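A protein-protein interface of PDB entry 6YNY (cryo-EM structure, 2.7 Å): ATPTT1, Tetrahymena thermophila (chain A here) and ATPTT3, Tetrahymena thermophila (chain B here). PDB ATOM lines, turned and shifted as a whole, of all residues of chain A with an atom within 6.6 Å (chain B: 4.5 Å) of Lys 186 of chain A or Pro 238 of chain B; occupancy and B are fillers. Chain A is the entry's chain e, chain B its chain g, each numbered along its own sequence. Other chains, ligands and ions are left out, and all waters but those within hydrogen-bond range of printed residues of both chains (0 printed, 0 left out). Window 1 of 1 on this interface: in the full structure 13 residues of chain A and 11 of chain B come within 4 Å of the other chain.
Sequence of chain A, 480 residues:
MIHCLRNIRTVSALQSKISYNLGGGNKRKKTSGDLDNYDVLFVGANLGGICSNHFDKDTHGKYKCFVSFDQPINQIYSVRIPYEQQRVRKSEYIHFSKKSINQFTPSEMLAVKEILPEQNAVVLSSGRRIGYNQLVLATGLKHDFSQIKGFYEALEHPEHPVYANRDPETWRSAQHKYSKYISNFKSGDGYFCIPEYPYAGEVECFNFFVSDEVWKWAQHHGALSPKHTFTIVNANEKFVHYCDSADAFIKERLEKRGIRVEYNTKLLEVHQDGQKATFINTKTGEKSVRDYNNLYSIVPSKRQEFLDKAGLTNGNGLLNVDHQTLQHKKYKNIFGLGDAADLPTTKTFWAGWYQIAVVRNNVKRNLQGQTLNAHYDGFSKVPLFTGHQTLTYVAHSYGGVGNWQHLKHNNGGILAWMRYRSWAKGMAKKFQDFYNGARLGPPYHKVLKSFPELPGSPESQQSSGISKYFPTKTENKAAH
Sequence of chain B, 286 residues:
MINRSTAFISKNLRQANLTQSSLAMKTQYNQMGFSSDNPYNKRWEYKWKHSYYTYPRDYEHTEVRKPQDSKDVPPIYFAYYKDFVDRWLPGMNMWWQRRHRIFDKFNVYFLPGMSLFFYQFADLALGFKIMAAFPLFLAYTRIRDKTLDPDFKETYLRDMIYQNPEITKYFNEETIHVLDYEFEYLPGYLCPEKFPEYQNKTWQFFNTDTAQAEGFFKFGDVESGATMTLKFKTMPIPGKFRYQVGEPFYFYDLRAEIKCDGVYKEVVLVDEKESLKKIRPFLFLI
Lys 186 of chain A touches three residues of chain B.
Pro 238 of chain B touches just one residue of chain A: Lys 186.
Of the printed residues of chain A, Phe 241 of chain B touches Asn 184 and Lys 186.
Printed residues of chain A within 4 Å of Arg 242 of chain B: Ser 183 and Lys 186.
Pro 281 of chain B touches none of the printed residues of chain A.
Ile 182 of chain A touches none of the printed residues of chain B.
The nearest printed residue of chain B that does not touch Lys 186 of chain A is Arg 280 of chain B (5.5 Å).
NZ of Lys 186 of chain A is in hydrogen-bond range of O of Arg 242 of chain B (2.5 Å).
Of the 14 printed residues of chain A, 4 touch a printed residue of chain B.
Among the printed residues, no Asp or Glu carboxylate lies within 4 Å of a Lys or Arg side-chain nitrogen of the other chain.
Among the printed residues, merely in contact across the chains: Ser 183 of chain A with Arg 242 of chain B, Asn 184 of chain A with Lys 240 of chain B, Asn 184 of chain A with Phe 241 of chain B, Lys 186 of chain A with Pro 238 of chain B, Lys 186 of chain A with Phe 241 of chain B and Ser 187 of chain A with Arg 280 of chain B.
O of Lys 186 of chain A sits at hydrogen-bond distance from N of Ser 225 of chain A (2.8 Å).
O of Ser 187 of chain A sits close to OD1 of Asn 293 of chain A (2.7 Å).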
ATOM      1  N   ILE A 182       6.037 -17.842   6.909  1.00  0.00           N
ATOM      2  CA  ILE A 182       6.226 -18.778   5.809  1.00  0.00           C
ATOM      3  C   ILE A 182       6.729 -20.121   6.318  1.00  0.00           C
ATOM      4  O   ILE A 182       6.336 -21.177   5.809  1.00  0.00           O
ATOM      5  CB  ILE A 182       7.185 -18.167   4.774  1.00  0.00           C
ATOM      6  CG1 ILE A 182       6.615 -16.849   4.256  1.00  0.00           C
ATOM      7  CG2 ILE A 182       7.424 -19.135   3.635  1.00  0.00           C
ATOM      8  CD1 ILE A 182       7.537 -16.106   3.345  1.00  0.00           C
ATOM      9  N   SER A 183       7.601 -20.106   7.324  1.00  0.00           N
ATOM     10  CA  SER A 183       8.169 -21.348   7.834  1.00  0.00           C
ATOM     11  C   SER A 183       7.110 -22.193   8.528  1.00  0.00           C
ATOM     12  O   SER A 183       6.924 -23.369   8.197  1.00  0.00           O
ATOM     13  CB  SER A 183       9.312 -21.035   8.794  1.00  0.00           C
ATOM     14  OG  SER A 183      10.232 -20.135   8.212  1.00  0.00           O
ATOM     15  N   ASN A 184       6.411 -21.610   9.499  1.00  0.00           N
ATOM     16  CA  ASN A 184       5.456 -22.352  10.319  1.00  0.00           C
ATOM     17  C   ASN A 184       4.065 -22.273   9.692  1.00  0.00           C
ATOM     18  O   ASN A 184       3.161 -21.582  10.163  1.00  0.00           O
ATOM     19  CB  ASN A 184       5.464 -21.821  11.746  1.00  0.00           C
ATOM     20  CG  ASN A 184       6.808 -21.981  12.416  1.00  0.00           C
ATOM     21  OD1 ASN A 184       7.807 -22.285  11.767  1.00  0.00           O
ATOM     22  ND2 ASN A 184       6.842 -21.775  13.723  1.00  0.00           N
ATOM     23  N   PHE A 185       3.914 -23.010   8.598  1.00  0.00           N
ATOM     24  CA  PHE A 185       2.643 -23.198   7.912  1.00  0.00           C
ATOM     25  C   PHE A 185       2.452 -24.672   7.597  1.00  0.00           C
ATOM     26  O   PHE A 185       2.136 -25.071   6.477  1.00  0.00           O
ATOM     27  CB  PHE A 185       2.557 -22.349   6.652  1.00  0.00           C
ATOM     28  CG  PHE A 185       1.268 -22.510   5.905  1.00  0.00           C
ATOM     29  CD1 PHE A 185       0.063 -22.528   6.578  1.00  0.00           C
ATOM     30  CD2 PHE A 185       1.259 -22.643   4.531  1.00  0.00           C
ATOM     31  CE1 PHE A 185      -1.118 -22.680   5.901  1.00  0.00           C
ATOM     32  CE2 PHE A 185       0.074 -22.793   3.850  1.00  0.00           C
ATOM     33  CZ  PHE A 185      -1.115 -22.810   4.536  1.00  0.00           C
ATOM     34  N   LYS A 186       2.677 -25.509   8.607  1.00  0.00           N
ATOM     35  CA  LYS A 186       2.683 -26.948   8.392  1.00  0.00           C
ATOM     36  C   LYS A 186       1.361 -27.448   7.832  1.00  0.00           C
ATOM     37  O   LYS A 186       1.338 -28.429   7.083  1.00  0.00           O
ATOM     38  CB  LYS A 186       3.003 -27.659   9.703  1.00  0.00           C
ATOM     39  CG  LYS A 186       4.289 -27.198  10.355  1.00  0.00           C
ATOM     40  CD  LYS A 186       5.467 -27.336   9.423  1.00  0.00           C
ATOM     41  CE  LYS A 186       6.761 -26.991  10.117  1.00  0.00           C
ATOM     42  NZ  LYS A 186       7.889 -27.011   9.162  1.00  0.00           N
ATOM     43  N   SER A 187       0.255 -26.800   8.175  1.00  0.00           N
ATOM     44  CA  SER A 187      -1.056 -27.245   7.720  1.00  0.00           C
ATOM     45  C   SER A 187      -2.073 -26.154   8.021  1.00  0.00           C
ATOM     46  O   SER A 187      -1.739 -25.090   8.554  1.00  0.00           O
ATOM     47  CB  SER A 187      -1.452 -28.557   8.390  1.00  0.00           C
ATOM     48  OG  SER A 187      -1.465 -28.406   9.797  1.00  0.00           O
ATOM     49  N   GLY A 188      -3.322 -26.432   7.675  1.00  0.00           N
ATOM     50  CA  GLY A 188      -4.426 -25.548   7.980  1.00  0.00           C
ATOM     51  C   GLY A 188      -4.772 -24.626   6.832  1.00  0.00           C
ATOM     52  O   GLY A 188      -4.269 -24.736   5.711  1.00  0.00           O
ATOM     53  N   GLY A 222       6.735 -33.122   2.175  1.00  0.00           N
ATOM     54  CA  GLY A 222       5.758 -33.439   3.192  1.00  0.00           C
ATOM     55  C   GLY A 222       5.698 -32.496   4.368  1.00  0.00           C
ATOM     56  O   GLY A 222       4.870 -32.706   5.262  1.00  0.00           O
ATOM     57  N   ALA A 223       6.541 -31.465   4.406  1.00  0.00           N
ATOM     58  CA  ALA A 223       6.506 -30.538   5.529  1.00  0.00           C
ATOM     59  C   ALA A 223       5.169 -29.821   5.613  1.00  0.00           C
ATOM     60  O   ALA A 223       4.734 -29.444   6.706  1.00  0.00           O
ATOM     61  CB  ALA A 223       7.645 -29.531   5.415  1.00  0.00           C
ATOM     62  N   LEU A 224       4.508 -29.626   4.479  1.00  0.00           N
ATOM     63  CA  LEU A 224       3.206 -28.983   4.419  1.00  0.00           C
ATOM     64  C   LEU A 224       2.157 -30.010   4.027  1.00  0.00           C
ATOM     65  O   LEU A 224       2.298 -30.693   3.008  1.00  0.00           O
ATOM     66  CB  LEU A 224       3.220 -27.828   3.419  1.00  0.00           C
ATOM     67  CG  LEU A 224       1.878 -27.226   3.013  1.00  0.00           C
ATOM     68  CD1 LEU A 224       1.104 -26.724   4.201  1.00  0.00           C
ATOM     69  CD2 LEU A 224       2.116 -26.102   2.041  1.00  0.00           C
ATOM     70  N   SER A 225       1.111 -30.113   4.838  1.00  0.00           N
ATOM     71  CA  SER A 225       0.062 -31.081   4.580  1.00  0.00           C
ATOM     72  C   SER A 225      -0.559 -30.832   3.207  1.00  0.00           C
ATOM     73  O   SER A 225      -0.619 -29.690   2.742  1.00  0.00           O
ATOM     74  CB  SER A 225      -1.009 -30.999   5.663  1.00  0.00           C
ATOM     75  OG  SER A 225      -2.042 -31.939   5.441  1.00  0.00           O
ATOM     76  N   PRO A 226      -1.031 -31.882   2.532  1.00  0.00           N
ATOM     77  CA  PRO A 226      -1.627 -31.681   1.207  1.00  0.00           C
ATOM     78  C   PRO A 226      -3.001 -31.049   1.263  1.00  0.00           C
ATOM     79  O   PRO A 226      -3.423 -30.442   0.271  1.00  0.00           O
ATOM     80  CB  PRO A 226      -1.686 -33.100   0.633  1.00  0.00           C
ATOM     81  CG  PRO A 226      -1.785 -33.966   1.809  1.00  0.00           C
ATOM     82  CD  PRO A 226      -0.984 -33.308   2.893  1.00  0.00           C
ATOM     83  N   HIS A 228      -4.384 -28.227   2.555  1.00  0.00           N
ATOM     84  CA  HIS A 228      -4.239 -26.871   3.049  1.00  0.00           C
ATOM     85  C   HIS A 228      -4.919 -25.940   2.059  1.00  0.00           C
ATOM     86  O   HIS A 228      -5.158 -26.300   0.904  1.00  0.00           O
ATOM     87  CB  HIS A 228      -2.767 -26.491   3.216  1.00  0.00           C
ATOM     88  CG  HIS A 228      -2.020 -26.404   1.924  1.00  0.00           C
ATOM     89  ND1 HIS A 228      -1.706 -25.203   1.328  1.00  0.00           N
ATOM     90  CD2 HIS A 228      -1.535 -27.368   1.107  1.00  0.00           C
ATOM     91  CE1 HIS A 228      -1.053 -25.430   0.202  1.00  0.00           C
ATOM     92  NE2 HIS A 228      -0.937 -26.736   0.045  1.00  0.00           N
ATOM     93  N   ASN A 293      -5.313 -21.007  10.251  1.00  0.00           N
ATOM     94  CA  ASN A 293      -4.121 -21.512  10.912  1.00  0.00           C
ATOM     95  C   ASN A 293      -2.877 -20.697  10.603  1.00  0.00           C
ATOM     96  O   ASN A 293      -1.860 -20.883  11.277  1.00  0.00           O
ATOM     97  CB  ASN A 293      -3.870 -22.973  10.518  1.00  0.00           C
ATOM     98  CG  ASN A 293      -2.727 -23.593  11.283  1.00  0.00           C
ATOM     99  OD1 ASN A 293      -1.587 -23.605  10.821  1.00  0.00           O
ATOM    100  ND2 ASN A 293      -3.024 -24.112  12.464  1.00  0.00           N
ATOM    101  N   ILE B 237       4.305 -34.935  15.629  1.00  0.00           N
ATOM    102  CA  ILE B 237       3.791 -33.634  15.207  1.00  0.00           C
ATOM    103  C   ILE B 237       4.929 -32.626  15.212  1.00  0.00           C
ATOM    104  O   ILE B 237       5.927 -32.791  15.932  1.00  0.00           O
ATOM    105  CB  ILE B 237       2.636 -33.154  16.114  1.00  0.00           C
ATOM    106  CG1 ILE B 237       3.098 -33.073  17.564  1.00  0.00           C
ATOM    107  CG2 ILE B 237       1.461 -34.084  16.001  1.00  0.00           C
ATOM    108  CD1 ILE B 237       2.185 -32.290  18.438  1.00  0.00           C
ATOM    109  N   PRO B 238       4.812 -31.569  14.415  1.00  0.00           N
ATOM    110  CA  PRO B 238       5.788 -30.483  14.467  1.00  0.00           C
ATOM    111  C   PRO B 238       5.425 -29.443  15.513  1.00  0.00           C
ATOM    112  O   PRO B 238       4.255 -29.177  15.789  1.00  0.00           O
ATOM    113  CB  PRO B 238       5.700 -29.889  13.056  1.00  0.00           C
ATOM    114  CG  PRO B 238       4.289 -30.105  12.671  1.00  0.00           C
ATOM    115  CD  PRO B 238       3.836 -31.371  13.331  1.00  0.00           C
ATOM    116  N   GLY B 239       6.459 -28.857  16.109  1.00  0.00           N
ATOM    117  CA  GLY B 239       6.234 -27.832  17.106  1.00  0.00           C
ATOM    118  C   GLY B 239       7.202 -26.669  17.094  1.00  0.00           C
ATOM    119  O   GLY B 239       8.412 -26.849  17.256  1.00  0.00           O
ATOM    120  N   LYS B 240       6.670 -25.465  16.895  1.00  0.00           N
ATOM    121  CA  LYS B 240       7.386 -24.223  17.163  1.00  0.00           C
ATOM    122  C   LYS B 240       8.625 -24.036  16.296  1.00  0.00           C
ATOM    123  O   LYS B 240       9.314 -23.019  16.416  1.00  0.00           O
ATOM    124  CB  LYS B 240       7.781 -24.162  18.640  1.00  0.00           C
ATOM    125  CG  LYS B 240       6.598 -24.170  19.596  1.00  0.00           C
ATOM    126  CD  LYS B 240       7.006 -24.514  21.021  1.00  0.00           C
ATOM    127  CE  LYS B 240       7.541 -23.313  21.779  1.00  0.00           C
ATOM    128  NZ  LYS B 240       8.773 -22.757  21.175  1.00  0.00           N
ATOM    129  N   PHE B 241       8.914 -24.989  15.415  1.00  0.00           N
ATOM    130  CA  PHE B 241      10.130 -24.954  14.619  1.00  0.00           C
ATOM    131  C   PHE B 241       9.821 -25.448  13.216  1.00  0.00           C
ATOM    132  O   PHE B 241       8.732 -25.953  12.933  1.00  0.00           O
ATOM    133  CB  PHE B 241      11.242 -25.787  15.260  1.00  0.00           C
ATOM    134  CG  PHE B 241      11.464 -25.476  16.707  1.00  0.00           C
ATOM    135  CD1 PHE B 241      11.847 -24.210  17.101  1.00  0.00           C
ATOM    136  CD2 PHE B 241      11.288 -26.446  17.676  1.00  0.00           C
ATOM    137  CE1 PHE B 241      12.040 -23.913  18.425  1.00  0.00           C
ATOM    138  CE2 PHE B 241      11.488 -26.150  19.007  1.00  0.00           C
ATOM    139  CZ  PHE B 241      11.867 -24.882  19.378  1.00  0.00           C
ATOM    140  N   ARG B 242      10.804 -25.301  12.333  1.00  0.00           N
ATOM    141  CA  ARG B 242      10.605 -25.562  10.914  1.00  0.00           C
ATOM    142  C   ARG B 242      10.959 -26.993  10.530  1.00  0.00           C
ATOM    143  O   ARG B 242      10.187 -27.659   9.834  1.00  0.00           O
ATOM    144  CB  ARG B 242      11.434 -24.576  10.090  1.00  0.00           C
ATOM    145  CG  ARG B 242      11.202 -24.671   8.602  1.00  0.00           C
ATOM    146  CD  ARG B 242      12.000 -23.631   7.858  1.00  0.00           C
ATOM    147  NE  ARG B 242      11.785 -23.704   6.419  1.00  0.00           N
ATOM    148  CZ  ARG B 242      12.363 -22.895   5.539  1.00  0.00           C
ATOM    149  NH1 ARG B 242      12.113 -23.032   4.246  1.00  0.00           N
ATOM    150  NH2 ARG B 242      13.190 -21.948   5.950  1.00  0.00           N
ATOM    151  N   GLY B 246       8.384 -31.788  17.126  1.00  0.00           N
ATOM    152  CA  GLY B 246       8.084 -31.289  18.450  1.00  0.00           C
ATOM    153  C   GLY B 246       7.837 -32.390  19.455  1.00  0.00           C
ATOM    154  O   GLY B 246       8.398 -32.381  20.554  1.00  0.00           O
ATOM    155  N   ILE B 279      -3.854 -30.127  14.020  1.00  0.00           N
ATOM    156  CA  ILE B 279      -2.466 -30.532  13.857  1.00  0.00           C
ATOM    157  C   ILE B 279      -2.416 -31.775  12.980  1.00  0.00           C
ATOM    158  O   ILE B 279      -3.326 -32.608  12.997  1.00  0.00           O
ATOM    159  CB  ILE B 279      -1.802 -30.784  15.227  1.00  0.00           C
ATOM    160  CG1 ILE B 279      -0.288 -30.914  15.087  1.00  0.00           C
ATOM    161  CG2 ILE B 279      -2.383 -32.018  15.878  1.00  0.00           C
ATOM    162  CD1 ILE B 279       0.400 -29.629  14.706  1.00  0.00           C
ATOM    163  N   ARG B 280      -1.343 -31.892  12.212  1.00  0.00           N
ATOM    164  CA  ARG B 280      -1.133 -32.977  11.269  1.00  0.00           C
ATOM    165  C   ARG B 280       0.201 -33.648  11.545  1.00  0.00           C
ATOM    166  O   ARG B 280       1.073 -33.069  12.202  1.00  0.00           O
ATOM    167  CB  ARG B 280      -1.167 -32.457   9.826  1.00  0.00           C
ATOM    168  CG  ARG B 280      -2.422 -31.689   9.465  1.00  0.00           C
ATOM    169  CD  ARG B 280      -3.671 -32.517   9.640  1.00  0.00           C
ATOM    170  NE  ARG B 280      -3.626 -33.751   8.866  1.00  0.00           N
ATOM    171  CZ  ARG B 280      -4.572 -34.679   8.896  1.00  0.00           C
ATOM    172  NH1 ARG B 280      -5.640 -34.517   9.658  1.00  0.00           N
ATOM    173  NH2 ARG B 280      -4.453 -35.771   8.160  1.00  0.00           N
ATOM    174  N   PRO B 281       0.394 -34.876  11.056  1.00  0.00           N
ATOM    175  CA  PRO B 281       1.645 -35.594  11.335  1.00  0.00           C
ATOM    176  C   PRO B 281       2.883 -34.923  10.758  1.00  0.00           C
ATOM    177  O   PRO B 281       2.785 -33.909  10.063  1.00  0.00           O
ATOM    178  CB  PRO B 281       1.406 -36.972  10.704  1.00  0.00           C
ATOM    179  CG  PRO B 281       0.260 -36.802   9.795  1.00  0.00           C
ATOM    180  CD  PRO B 281      -0.583 -35.734  10.375  1.00  0.00           C
ATOM    181  N   PHE B 282       4.053 -35.497  11.040  1.00  0.00           N
ATOM    182  CA  PHE B 282       5.333 -34.868  10.742  1.00  0.00           C
ATOM    183  C   PHE B 282       6.034 -35.437   9.516  1.00  0.00           C
ATOM    184  O   PHE B 282       6.761 -34.702   8.842  1.00  0.00           O
ATOM    185  CB  PHE B 282       6.266 -34.995  11.944  1.00  0.00           C
ATOM    186  CG  PHE B 282       7.601 -34.361  11.739  1.00  0.00           C
ATOM    187  CD1 PHE B 282       7.746 -32.995  11.827  1.00  0.00           C
ATOM    188  CD2 PHE B 282       8.711 -35.130  11.466  1.00  0.00           C
ATOM    189  CE1 PHE B 282       8.967 -32.409  11.642  1.00  0.00           C
ATOM    190  CE2 PHE B 282       9.937 -34.545  11.280  1.00  0.00           C
ATOM    191  CZ  PHE B 282      10.064 -33.184  11.368  1.00  0.00           C
